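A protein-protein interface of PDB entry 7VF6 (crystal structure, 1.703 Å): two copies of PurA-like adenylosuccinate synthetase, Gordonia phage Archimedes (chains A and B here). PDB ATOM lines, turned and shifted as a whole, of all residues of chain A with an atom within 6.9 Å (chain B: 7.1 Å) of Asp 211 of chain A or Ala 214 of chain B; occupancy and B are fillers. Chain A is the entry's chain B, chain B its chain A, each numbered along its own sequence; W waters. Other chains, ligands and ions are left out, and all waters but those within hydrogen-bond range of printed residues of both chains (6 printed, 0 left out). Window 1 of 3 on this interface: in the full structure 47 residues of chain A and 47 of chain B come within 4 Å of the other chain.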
ATOM      1  N   VAL A  41     -13.878 -15.794  10.958  1.00  0.00           N
ATOM      2  CA  VAL A  41     -13.480 -15.147   9.716  1.00  0.00           C
ATOM      3  C   VAL A  41     -14.731 -14.982   8.859  1.00  0.00           C
ATOM      4  O   VAL A  41     -15.793 -15.522   9.168  1.00  0.00           O
ATOM      5  CB  VAL A  41     -12.409 -15.959   8.958  1.00  0.00           C
ATOM      6  CG1 VAL A  41     -11.106 -16.055   9.778  1.00  0.00           C
ATOM      7  CG2 VAL A  41     -12.938 -17.351   8.649  1.00  0.00           C
ATOM      8  N   GLY A  78      -9.779 -10.534   7.714  1.00  0.00           N
ATOM      9  CA  GLY A  78     -10.558 -11.004   6.580  1.00  0.00           C
ATOM     10  C   GLY A  78     -11.992 -11.313   6.972  1.00  0.00           C
ATOM     11  O   GLY A  78     -12.445 -12.460   6.873  1.00  0.00           O
ATOM     12  N   TYR A 190     -17.446 -26.421   1.421  1.00  0.00           N
ATOM     13  CA  TYR A 190     -16.621 -26.475   0.215  1.00  0.00           C
ATOM     14  C   TYR A 190     -17.436 -26.237  -1.053  1.00  0.00           C
ATOM     15  O   TYR A 190     -17.045 -25.450  -1.928  1.00  0.00           O
ATOM     16  CB  TYR A 190     -15.920 -27.830   0.120  1.00  0.00           C
ATOM     17  CG  TYR A 190     -15.207 -27.964  -1.205  1.00  0.00           C
ATOM     18  CD1 TYR A 190     -14.083 -27.202  -1.478  1.00  0.00           C
ATOM     19  CD2 TYR A 190     -15.692 -28.803  -2.198  1.00  0.00           C
ATOM     20  CE1 TYR A 190     -13.437 -27.294  -2.697  1.00  0.00           C
ATOM     21  CE2 TYR A 190     -15.059 -28.898  -3.414  1.00  0.00           C
ATOM     22  CZ  TYR A 190     -13.928 -28.149  -3.658  1.00  0.00           C
ATOM     23  OH  TYR A 190     -13.290 -28.241  -4.879  1.00  0.00           O
ATOM     24  N   HIS A 195     -15.224 -20.938  -6.713  1.00  0.00           N
ATOM     25  CA  HIS A 195     -14.546 -21.684  -7.769  1.00  0.00           C
ATOM     26  C   HIS A 195     -14.699 -23.196  -7.637  1.00  0.00           C
ATOM     27  O   HIS A 195     -14.011 -23.933  -8.352  1.00  0.00           O
ATOM     28  CB  HIS A 195     -13.052 -21.342  -7.805  1.00  0.00           C
ATOM     29  CG  HIS A 195     -12.751 -19.897  -8.069  1.00  0.00           C
ATOM     30  ND1 HIS A 195     -12.755 -18.941  -7.073  1.00  0.00           N
ATOM     31  CD2 HIS A 195     -12.375 -19.257  -9.205  1.00  0.00           C
ATOM     32  CE1 HIS A 195     -12.424 -17.770  -7.591  1.00  0.00           C
ATOM     33  NE2 HIS A 195     -12.189 -17.935  -8.883  1.00  0.00           N
ATOM     34  N   SER A 205     -17.256 -16.266  -1.845  1.00  0.00           N
ATOM     35  CA  SER A 205     -15.852 -16.567  -1.593  1.00  0.00           C
ATOM     36  C   SER A 205     -15.653 -18.067  -1.747  1.00  0.00           C
ATOM     37  O   SER A 205     -16.600 -18.817  -1.986  1.00  0.00           O
ATOM     38  CB  SER A 205     -15.399 -16.094  -0.202  1.00  0.00           C
ATOM     39  OG  SER A 205     -15.844 -16.997   0.793  1.00  0.00           O
ATOM     40  N   ASP A 206     -14.409 -18.504  -1.617  1.00  0.00           N
ATOM     41  CA  ASP A 206     -14.177 -19.935  -1.495  1.00  0.00           C
ATOM     42  C   ASP A 206     -14.134 -20.318  -0.018  1.00  0.00           C
ATOM     43  O   ASP A 206     -14.012 -19.466   0.861  1.00  0.00           O
ATOM     44  CB  ASP A 206     -12.905 -20.331  -2.244  1.00  0.00           C
ATOM     45  CG  ASP A 206     -13.113 -20.293  -3.764  1.00  0.00           C
ATOM     46  OD1 ASP A 206     -13.771 -21.222  -4.303  1.00  0.00           O
ATOM     47  OD2 ASP A 206     -12.648 -19.318  -4.397  1.00  0.00           O
ATOM     48  N   ALA A 207     -14.307 -21.610   0.256  1.00  0.00           N
ATOM     49  CA  ALA A 207     -14.594 -22.033   1.621  1.00  0.00           C
ATOM     50  C   ALA A 207     -13.702 -23.192   2.035  1.00  0.00           C
ATOM     51  O   ALA A 207     -14.146 -24.125   2.708  1.00  0.00           O
ATOM     52  CB  ALA A 207     -16.070 -22.398   1.773  1.00  0.00           C
ATOM     53  N   ARG A 208     -12.432 -23.156   1.626  1.00  0.00           N
ATOM     54  CA  ARG A 208     -11.425 -24.137   2.011  1.00  0.00           C
ATOM     55  C   ARG A 208     -10.627 -23.615   3.198  1.00  0.00           C
ATOM     56  O   ARG A 208     -10.597 -22.409   3.464  1.00  0.00           O
ATOM     57  CB  ARG A 208     -10.464 -24.418   0.849  1.00  0.00           C
ATOM     58  CG  ARG A 208     -11.134 -24.846  -0.452  1.00  0.00           C
ATOM     59  CD  ARG A 208     -10.229 -24.551  -1.651  1.00  0.00           C
ATOM     60  NE  ARG A 208     -10.074 -23.106  -1.794  1.00  0.00           N
ATOM     61  CZ  ARG A 208      -9.459 -22.501  -2.804  1.00  0.00           C
ATOM     62  NH1 ARG A 208      -8.936 -23.220  -3.787  1.00  0.00           N
ATOM     63  NH2 ARG A 208      -9.392 -21.173  -2.838  1.00  0.00           N
ATOM     64  N   ALA A 209      -9.930 -24.535   3.881  1.00  0.00           N
ATOM     65  CA  ALA A 209      -9.070 -24.127   4.989  1.00  0.00           C
ATOM     66  C   ALA A 209      -8.125 -23.004   4.576  1.00  0.00           C
ATOM     67  O   ALA A 209      -7.966 -22.020   5.305  1.00  0.00           O
ATOM     68  CB  ALA A 209      -8.283 -25.331   5.524  1.00  0.00           C
ATOM     69  N   ILE A 210      -7.512 -23.113   3.393  1.00  0.00           N
ATOM     70  CA  ILE A 210      -6.524 -22.108   3.012  1.00  0.00           C
ATOM     71  C   ILE A 210      -7.172 -20.730   2.854  1.00  0.00           C
ATOM     72  O   ILE A 210      -6.533 -19.710   3.126  1.00  0.00           O
ATOM     73  CB  ILE A 210      -5.774 -22.546   1.738  1.00  0.00           C
ATOM     74  CG1 ILE A 210      -4.513 -21.702   1.558  1.00  0.00           C
ATOM     75  CG2 ILE A 210      -6.676 -22.476   0.506  1.00  0.00           C
ATOM     76  CD1 ILE A 210      -3.554 -22.252   0.488  1.00  0.00           C
ATOM     77  N   ASP A 211      -8.434 -20.676   2.417  1.00  0.00           N
ATOM     78  CA  ASP A 211      -9.135 -19.391   2.339  1.00  0.00           C
ATOM     79  C   ASP A 211      -9.311 -18.778   3.720  1.00  0.00           C
ATOM     80  O   ASP A 211      -9.133 -17.570   3.904  1.00  0.00           O
ATOM     81  CB  ASP A 211     -10.508 -19.564   1.687  1.00  0.00           C
ATOM     82  CG  ASP A 211     -10.421 -20.207   0.326  1.00  0.00           C
ATOM     83  OD1 ASP A 211      -9.810 -19.590  -0.568  1.00  0.00           O
ATOM     84  OD2 ASP A 211     -10.937 -21.339   0.156  1.00  0.00           O
ATOM     85  N   PHE A 212      -9.694 -19.595   4.697  1.00  0.00           N
ATOM     86  CA  PHE A 212      -9.921 -19.077   6.039  1.00  0.00           C
ATOM     87  C   PHE A 212      -8.615 -18.683   6.714  1.00  0.00           C
ATOM     88  O   PHE A 212      -8.585 -17.725   7.499  1.00  0.00           O
ATOM     89  CB  PHE A 212     -10.678 -20.120   6.845  1.00  0.00           C
ATOM     90  CG  PHE A 212     -12.008 -20.496   6.234  1.00  0.00           C
ATOM     91  CD1 PHE A 212     -12.817 -19.529   5.649  1.00  0.00           C
ATOM     92  CD2 PHE A 212     -12.434 -21.815   6.227  1.00  0.00           C
ATOM     93  CE1 PHE A 212     -14.051 -19.878   5.071  1.00  0.00           C
ATOM     94  CE2 PHE A 212     -13.657 -22.173   5.653  1.00  0.00           C
ATOM     95  CZ  PHE A 212     -14.462 -21.202   5.080  1.00  0.00           C
ATOM     96  N   LEU A 213      -7.531 -19.404   6.419  1.00  0.00           N
ATOM     97  CA  LEU A 213      -6.223 -19.018   6.937  1.00  0.00           C
ATOM     98  C   LEU A 213      -5.773 -17.690   6.345  1.00  0.00           C
ATOM     99  O   LEU A 213      -5.205 -16.847   7.055  1.00  0.00           O
ATOM    100  CB  LEU A 213      -5.201 -20.113   6.635  1.00  0.00           C
ATOM    101  CG  LEU A 213      -5.407 -21.394   7.458  1.00  0.00           C
ATOM    102  CD1 LEU A 213      -4.770 -22.600   6.763  1.00  0.00           C
ATOM    103  CD2 LEU A 213      -4.823 -21.245   8.867  1.00  0.00           C
ATOM    104  N   ALA A 214      -5.985 -17.497   5.039  1.00  0.00           N
ATOM    105  CA  ALA A 214      -5.695 -16.200   4.439  1.00  0.00           C
ATOM    106  C   ALA A 214      -6.498 -15.081   5.110  1.00  0.00           C
ATOM    107  O   ALA A 214      -5.951 -14.006   5.385  1.00  0.00           O
ATOM    108  CB  ALA A 214      -5.972 -16.235   2.935  1.00  0.00           C
ATOM    109  N   MET A 215      -7.793 -15.306   5.365  1.00  0.00           N
ATOM    110  CA  MET A 215      -8.602 -14.306   6.073  1.00  0.00           C
ATOM    111  C   MET A 215      -8.067 -14.059   7.476  1.00  0.00           C
ATOM    112  O   MET A 215      -8.097 -12.926   7.984  1.00  0.00           O
ATOM    113  CB  MET A 215     -10.060 -14.762   6.161  1.00  0.00           C
ATOM    114  CG  MET A 215     -10.756 -14.882   4.818  1.00  0.00           C
ATOM    115  SD  MET A 215     -12.404 -15.604   5.013  1.00  0.00           S
ATOM    116  CE  MET A 215     -12.750 -16.062   3.315  1.00  0.00           C
ATOM    117  N   ALA A 216      -7.614 -15.118   8.136  1.00  0.00           N
ATOM    118  CA  ALA A 216      -7.106 -14.976   9.492  1.00  0.00           C
ATOM    119  C   ALA A 216      -5.795 -14.206   9.524  1.00  0.00           C
ATOM    120  O   ALA A 216      -5.476 -13.575  10.539  1.00  0.00           O
ATOM    121  CB  ALA A 216      -6.919 -16.351  10.126  1.00  0.00           C
ATOM    122  N   VAL B  41      -1.483 -16.534 -11.575  1.00  0.00           N
ATOM    123  CA  VAL B  41      -2.716 -16.344 -10.827  1.00  0.00           C
ATOM    124  C   VAL B  41      -3.096 -14.871 -10.922  1.00  0.00           C
ATOM    125  O   VAL B  41      -2.313 -14.033 -11.372  1.00  0.00           O
ATOM    126  CB  VAL B  41      -2.581 -16.771  -9.347  1.00  0.00           C
ATOM    127  CG1 VAL B  41      -2.271 -18.267  -9.226  1.00  0.00           C
ATOM    128  CG2 VAL B  41      -1.478 -15.959  -8.680  1.00  0.00           C
ATOM    129  N   ALA B  76      -4.564 -20.183 -13.539  1.00  0.00           N
ATOM    130  CA  ALA B  76      -5.254 -20.810 -12.418  1.00  0.00           C
ATOM    131  C   ALA B  76      -6.733 -20.444 -12.366  1.00  0.00           C
ATOM    132  O   ALA B  76      -7.179 -19.438 -12.930  1.00  0.00           O
ATOM    133  CB  ALA B  76      -4.600 -20.402 -11.096  1.00  0.00           C
ATOM    134  N   ALA B  77      -7.492 -21.265 -11.628  1.00  0.00           N
ATOM    135  CA  ALA B  77      -8.902 -20.965 -11.398  1.00  0.00           C
ATOM    136  C   ALA B  77      -9.079 -19.580 -10.779  1.00  0.00           C
ATOM    137  O   ALA B  77      -9.993 -18.840 -11.160  1.00  0.00           O
ATOM    138  CB  ALA B  77      -9.544 -22.037 -10.510  1.00  0.00           C
ATOM    139  N   GLY B  78      -8.209 -19.213  -9.828  1.00  0.00           N
ATOM    140  CA  GLY B  78      -8.262 -17.903  -9.186  1.00  0.00           C
ATOM    141  C   GLY B  78      -7.588 -16.841 -10.031  1.00  0.00           C
ATOM    142  O   GLY B  78      -6.590 -16.230  -9.627  1.00  0.00           O
ATOM    143  N   ARG B 208      -0.098 -11.951  -0.588  1.00  0.00           N
ATOM    144  CA  ARG B 208       0.790 -12.867   0.117  1.00  0.00           C
ATOM    145  C   ARG B 208       0.829 -14.226  -0.579  1.00  0.00           C
ATOM    146  O   ARG B 208      -0.060 -14.584  -1.361  1.00  0.00           O
ATOM    147  CB  ARG B 208       0.325 -13.067   1.566  1.00  0.00           C
ATOM    148  CG  ARG B 208       0.105 -11.784   2.357  1.00  0.00           C
ATOM    149  CD  ARG B 208      -0.889 -12.008   3.498  1.00  0.00           C
ATOM    150  NE  ARG B 208      -2.227 -12.271   2.965  1.00  0.00           N
ATOM    151  CZ  ARG B 208      -3.330 -12.419   3.698  1.00  0.00           C
ATOM    152  NH1 ARG B 208      -3.271 -12.321   5.016  1.00  0.00           N
ATOM    153  NH2 ARG B 208      -4.498 -12.651   3.103  1.00  0.00           N
ATOM    154  N   ALA B 209       1.867 -15.008  -0.253  1.00  0.00           N
ATOM    155  CA  ALA B 209       1.961 -16.353  -0.811  1.00  0.00           C
ATOM    156  C   ALA B 209       0.670 -17.137  -0.602  1.00  0.00           C
ATOM    157  O   ALA B 209       0.189 -17.813  -1.522  1.00  0.00           O
ATOM    158  CB  ALA B 209       3.159 -17.097  -0.204  1.00  0.00           C
ATOM    159  N   ILE B 210       0.082 -17.059   0.598  1.00  0.00           N
ATOM    160  CA  ILE B 210      -1.099 -17.872   0.866  1.00  0.00           C
ATOM    161  C   ILE B 210      -2.268 -17.440  -0.026  1.00  0.00           C
ATOM    162  O   ILE B 210      -3.104 -18.268  -0.402  1.00  0.00           O
ATOM    163  CB  ILE B 210      -1.460 -17.835   2.365  1.00  0.00           C
ATOM    164  CG1 ILE B 210      -2.454 -18.961   2.686  1.00  0.00           C
ATOM    165  CG2 ILE B 210      -1.995 -16.454   2.789  1.00  0.00           C
ATOM    166  CD1 ILE B 210      -2.672 -19.212   4.198  1.00  0.00           C
ATOM    167  N   ASP B 211      -2.337 -16.156  -0.400  1.00  0.00           N
ATOM    168  CA  ASP B 211      -3.389 -15.732  -1.322  1.00  0.00           C
ATOM    169  C   ASP B 211      -3.204 -16.368  -2.688  1.00  0.00           C
ATOM    170  O   ASP B 211      -4.172 -16.815  -3.313  1.00  0.00           O
ATOM    171  CB  ASP B 211      -3.399 -14.210  -1.471  1.00  0.00           C
ATOM    172  CG  ASP B 211      -3.558 -13.509  -0.150  1.00  0.00           C
ATOM    173  OD1 ASP B 211      -4.642 -13.656   0.458  1.00  0.00           O
ATOM    174  OD2 ASP B 211      -2.598 -12.830   0.288  1.00  0.00           O
ATOM    175  N   PHE B 212      -1.963 -16.406  -3.168  1.00  0.00           N
ATOM    176  CA  PHE B 212      -1.706 -16.947  -4.495  1.00  0.00           C
ATOM    177  C   PHE B 212      -1.867 -18.456  -4.512  1.00  0.00           C
ATOM    178  O   PHE B 212      -2.282 -19.023  -5.530  1.00  0.00           O
ATOM    179  CB  PHE B 212      -0.308 -16.535  -4.939  1.00  0.00           C
ATOM    180  CG  PHE B 212      -0.116 -15.043  -4.982  1.00  0.00           C
ATOM    181  CD1 PHE B 212      -1.133 -14.216  -5.437  1.00  0.00           C
ATOM    182  CD2 PHE B 212       1.073 -14.469  -4.554  1.00  0.00           C
ATOM    183  CE1 PHE B 212      -0.968 -12.819  -5.467  1.00  0.00           C
ATOM    184  CE2 PHE B 212       1.250 -13.091  -4.577  1.00  0.00           C
ATOM    185  CZ  PHE B 212       0.230 -12.265  -5.040  1.00  0.00           C
ATOM    186  N   LEU B 213      -1.576 -19.116  -3.391  1.00  0.00           N
ATOM    187  CA  LEU B 213      -1.804 -20.554  -3.299  1.00  0.00           C
ATOM    188  C   LEU B 213      -3.295 -20.870  -3.303  1.00  0.00           C
ATOM    189  O   LEU B 213      -3.733 -21.834  -3.953  1.00  0.00           O
ATOM    190  CB  LEU B 213      -1.125 -21.101  -2.035  1.00  0.00           C
ATOM    191  CG  LEU B 213       0.414 -21.111  -2.066  1.00  0.00           C
ATOM    192  CD1 LEU B 213       1.020 -21.043  -0.669  1.00  0.00           C
ATOM    193  CD2 LEU B 213       0.922 -22.360  -2.788  1.00  0.00           C
ATOM    194  N   ALA B 214      -4.095 -20.070  -2.588  1.00  0.00           N
ATOM    195  CA  ALA B 214      -5.541 -20.241  -2.649  1.00  0.00           C
ATOM    196  C   ALA B 214      -6.062 -20.060  -4.079  1.00  0.00           C
ATOM    197  O   ALA B 214      -6.913 -20.832  -4.534  1.00  0.00           O
ATOM    198  CB  ALA B 214      -6.224 -19.264  -1.690  1.00  0.00           C
ATOM    199  N   MET B 215      -5.567 -19.043  -4.798  1.00  0.00           N
ATOM    200  CA  MET B 215      -5.950 -18.865  -6.201  1.00  0.00           C
ATOM    201  C   MET B 215      -5.515 -20.049  -7.048  1.00  0.00           C
ATOM    202  O   MET B 215      -6.225 -20.458  -7.975  1.00  0.00           O
ATOM    203  CB  MET B 215      -5.335 -17.587  -6.775  1.00  0.00           C
ATOM    204  CG  MET B 215      -5.784 -16.318  -6.085  1.00  0.00           C
ATOM    205  SD  MET B 215      -4.879 -14.895  -6.752  1.00  0.00           S
ATOM    206  CE  MET B 215      -5.302 -13.648  -5.527  1.00  0.00           C
ATOM    207  N   ALA B 216      -4.321 -20.583  -6.777  1.00  0.00           N
ATOM    208  CA  ALA B 216      -3.830 -21.725  -7.543  1.00  0.00           C
ATOM    209  C   ALA B 216      -4.658 -22.976  -7.294  1.00  0.00           C
ATOM    210  O   ALA B 216      -4.749 -23.843  -8.177  1.00  0.00           O
ATOM    211  CB  ALA B 216      -2.370 -21.993  -7.202  1.00  0.00           C
ATOM    212  N   GLY B 217      -5.277 -23.094  -6.121  1.00  0.00           N
ATOM    213  CA  GLY B 217      -5.965 -24.325  -5.797  1.00  0.00           C
ATOM    214  C   GLY B 217      -5.039 -25.445  -5.384  1.00  0.00           C
ATOM    215  O   GLY B 217      -5.442 -26.612  -5.405  1.00  0.00           O
ATOM    216  N   ILE B 218      -3.808 -25.119  -5.003  1.00  0.00           N
ATOM    217  CA  ILE B 218      -2.812 -26.084  -4.546  1.00  0.00           C
ATOM    218  C   ILE B 218      -2.402 -25.700  -3.135  1.00  0.00           C
ATOM    219  O   ILE B 218      -2.142 -24.522  -2.866  1.00  0.00           O
ATOM    220  CB  ILE B 218      -1.573 -26.098  -5.472  1.00  0.00           C
ATOM    221  CG1 ILE B 218      -1.943 -26.532  -6.898  1.00  0.00           C
ATOM    222  CG2 ILE B 218      -0.463 -26.966  -4.871  1.00  0.00           C
ATOM    223  CD1 ILE B 218      -2.482 -27.938  -7.004  1.00  0.00           C
ATOM    224  N   ASN B 219      -2.313 -26.701  -2.232  1.00  0.00           N
ATOM    225  CA  ASN B 219      -1.892 -26.399  -0.857  1.00  0.00           C
ATOM    226  C   ASN B 219      -0.437 -26.777  -0.642  1.00  0.00           C
ATOM    227  O   ASN B 219      -0.014 -27.853  -1.064  1.00  0.00           O
ATOM    228  CB  ASN B 219      -2.722 -27.175   0.167  1.00  0.00           C
ATOM    229  CG  ASN B 219      -4.197 -27.001  -0.020  1.00  0.00           C
ATOM    230  OD1 ASN B 219      -4.729 -25.897   0.138  1.00  0.00           O
ATOM    231  ND2 ASN B 219      -4.888 -28.100  -0.349  1.00  0.00           N
ATOM    232  N   PRO B 220       0.362 -25.968   0.056  1.00  0.00           N
ATOM    233  CA  PRO B 220       1.735 -26.405   0.356  1.00  0.00           C
ATOM    234  C   PRO B 220       1.776 -27.727   1.109  1.00  0.00           C
ATOM    235  O   PRO B 220       2.717 -28.516   0.926  1.00  0.00           O
ATOM    236  CB  PRO B 220       2.290 -25.243   1.196  1.00  0.00           C
ATOM    237  CG  PRO B 220       1.461 -24.033   0.755  1.00  0.00           C
ATOM    238  CD  PRO B 220       0.084 -24.607   0.548  1.00  0.00           C
ATOM    239  N   TRP B 221       0.780 -27.998   1.958  1.00  0.00           N
ATOM    240  CA  TRP B 221       0.754 -29.258   2.683  1.00  0.00           C
ATOM    241  C   TRP B 221       0.239 -30.421   1.834  1.00  0.00           C
ATOM    242  O   TRP B 221       0.074 -31.521   2.361  1.00  0.00           O
ATOM    243  CB  TRP B 221      -0.066 -29.116   3.974  1.00  0.00           C
ATOM    244  CG  TRP B 221      -1.423 -28.504   3.815  1.00  0.00           C
ATOM    245  CD1 TRP B 221      -2.599 -29.159   3.585  1.00  0.00           C
ATOM    246  CD2 TRP B 221      -1.742 -27.116   3.898  1.00  0.00           C
ATOM    247  NE1 TRP B 221      -3.630 -28.255   3.504  1.00  0.00           N
ATOM    248  CE2 TRP B 221      -3.131 -26.994   3.707  1.00  0.00           C
ATOM    249  CE3 TRP B 221      -0.989 -25.961   4.142  1.00  0.00           C
ATOM    250  CZ2 TRP B 221      -3.781 -25.765   3.717  1.00  0.00           C
ATOM    251  CZ3 TRP B 221      -1.635 -24.741   4.150  1.00  0.00           C
ATOM    252  CH2 TRP B 221      -3.022 -24.653   3.952  1.00  0.00           C
HETATM  253  O   HOH W   1      -6.985 -25.683   1.993  1.00  0.00           O
HETATM  254  O   HOH W   2      -8.641 -21.802  -6.758  1.00  0.00           O
HETATM  255  O   HOH W   3      -9.852 -19.708  -5.874  1.00  0.00           O
HETATM  256  O   HOH W   4     -11.287 -15.836 -10.258  1.00  0.00           O
HETATM  257  O   HOH W   5      -6.013 -11.204   6.559  1.00  0.00           O
HETATM  258  O   HOH W   6      -7.083 -10.914   4.349  1.00  0.00           O
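Among the printed residues, pairs that only touch across the chains: Ile 210 of chain A with Ile 210 of chain B, Leu 213 of chain A with Ile 210 of chain B, Ile 210 of chain A with Leu 213 of chain B, Arg 208 of chain A with Gly 217 of chain B, Asp 211 of chain A with Ala 214 of chain B, Ile 210 of chain A with Ala 214 of chain B, Ala 214 of chain A with Asp 211 of chain B, Ala 214 of chain A with Ile 210 of chain B, Ile 210 of chain A with Asn 219 of chain B, Leu 213 of chain A with Trp 221 of chain B and His 195 of chain A with Gly 78 of chain B.
Of the 18 printed residues of chain B, 10 touch a printed residue of chain A. Printed residues of chain B that touch a printed residue of chain A: Ala 77, Gly 78, Arg 208, Ile 210, Asp 211, Leu 213, Ala 214, Gly 217, Asn 219 and Trp 221. Hydrophobic or aromatic side chains of chain B that line the printed part of chain A: Ile 210, Leu 213, Ala 214 and Trp 221. Along chain B the printed residues that touch a printed residue of chain A span positions 77 to 221.
Arg 208 of chain A touches Ala 214 of chain B, and with the chains exchanged Ala 214 of chain A touches Arg 208 of chain B. Ile 210 of chain A touches Leu 213 of chain B, and with the chains exchanged Leu 213 of chain A touches Ile 210 of chain B. Ile 210 of chain A touches Ala 214 of chain B, and with the chains exchanged Ala 214 of chain A touches Ile 210 of chain B. Asp 211 of chain A touches Ala 214 of chain B, and with the chains exchanged Ala 214 of chain A touches Asp 211 of chain B. Positions printed for both chains: 41, 78, 208, 209, 210, 211, 212, 213, 214, 215 and 216.
Water W4 bridges a ring nitrogen (NE2) of His 195 of chain A (2.7 Å) and the backbone carbonyl oxygen of Ala 77 of chain B (3.4 Å). Water W1 bridges OD1 of Asn 219 of chain B and N of Ile 210 of chain A. Water W2 lies within hydrogen-bond range of the backbone carbonyl oxygen (O) of Ala 214 of chain B (3.0 Å), the backbone carbonyl oxygen (O) of Met 215 of chain B (3.0 Å) and the guanidinium group (NH1) of Arg 208 of chain A (3.3 Å). Water W5 lies within hydrogen-bond range of the backbone carbonyl oxygen (O) of Ala 214 of chain A, the backbone carbonyl oxygen (O) of Met 215 of chain A and the guanidinium group (NH1) of Arg 208 of chain B. Water W3 lies within hydrogen-bond range of OD2 of Asp 206 of chain A (3.2 Å), ND1 of His 195 of chain A (3.2 Å), NH2 of Arg 208 of chain A (3.4 Å) and O of Ala 214 of chain B (3.4 Å). Water W6 lies within hydrogen-bond range of the guanidinium group of Arg 208 of chain B (3.4 Å) and the backbone carbonyl oxygen of Ala 214 of chain A (3.5 Å).
NE2 of His 195 of chain A sits close to O of Ala 77 of chain B, 3.3 Å away. The backbone carbonyl oxygen (O) of Ala 214 of chain A is in hydrogen-bond range of the guanidinium group (NH2) of Arg 208 of chain B (3.0 Å). NH2 of Arg 208 of chain A lies within hydrogen-bond range of O of Ala 214 of chain B.
Of the printed residues of chain B, Asp 211 of chain A touches Ala 214 (3.8 Å). Ala 214 of chain B touches just these residues of chain A: Arg 208 (3.0 Å), Ile 210 (3.8 Å) and Asp 211 (3.8 Å). Of the printed residues of chain A, Trp 221 of chain B touches Leu 213. Of the printed residues of chain A, Leu 213 of chain B touches Ile 210. Of the printed residues of chain A, Gly 78 of chain B touches His 195. Printed residues of chain B within 4 Å of Arg 208 of chain A: Ala 214 (3.0 Å) and Gly 217 (3.8 Å). Pro 220 of chain B touches none of the printed residues of chain A. Asp 206 of chain A touches none of the printed residues of chain B. The nearest residue of chain B that does not touch Asp 211 of chain A is Met 215 of chain B (6.0 Å). The nearest printed residue of chain A that does not touch Gly 78 of chain B is Asp 206 of chain A (6.6 Å).
The backbone NH of Gly 78 of chain B sits at hydrogen-bond distance from the backbone carbonyl oxygen of Met 215 of chain B. The guanidinium group (NE) of Arg 208 of chain B is in salt-bridge range of the side-chain carboxylate (OD2) of Asp 211 of chain B (2.8 Å). The backbone carbonyl oxygen (O) of Leu 213 of chain B lies within hydrogen-bond range of the backbone NH (N) of Ile 218 of chain B. A ring nitrogen (ND1) of His 195 of chain A lies within hydrogen-bond range of the side-chain carboxylate (OD2) of Asp 206 of chain A (2.7 Å). OD2 of Asp 211 of chain A is in hydrogen-bond range of N of Ala 207 of chain A (3.4 Å). The side-chain carboxylate (OD2) of Asp 211 of chain A is in salt-bridge range of the guanidinium group (NE) of Arg 208 of chain A (2.8 Å).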
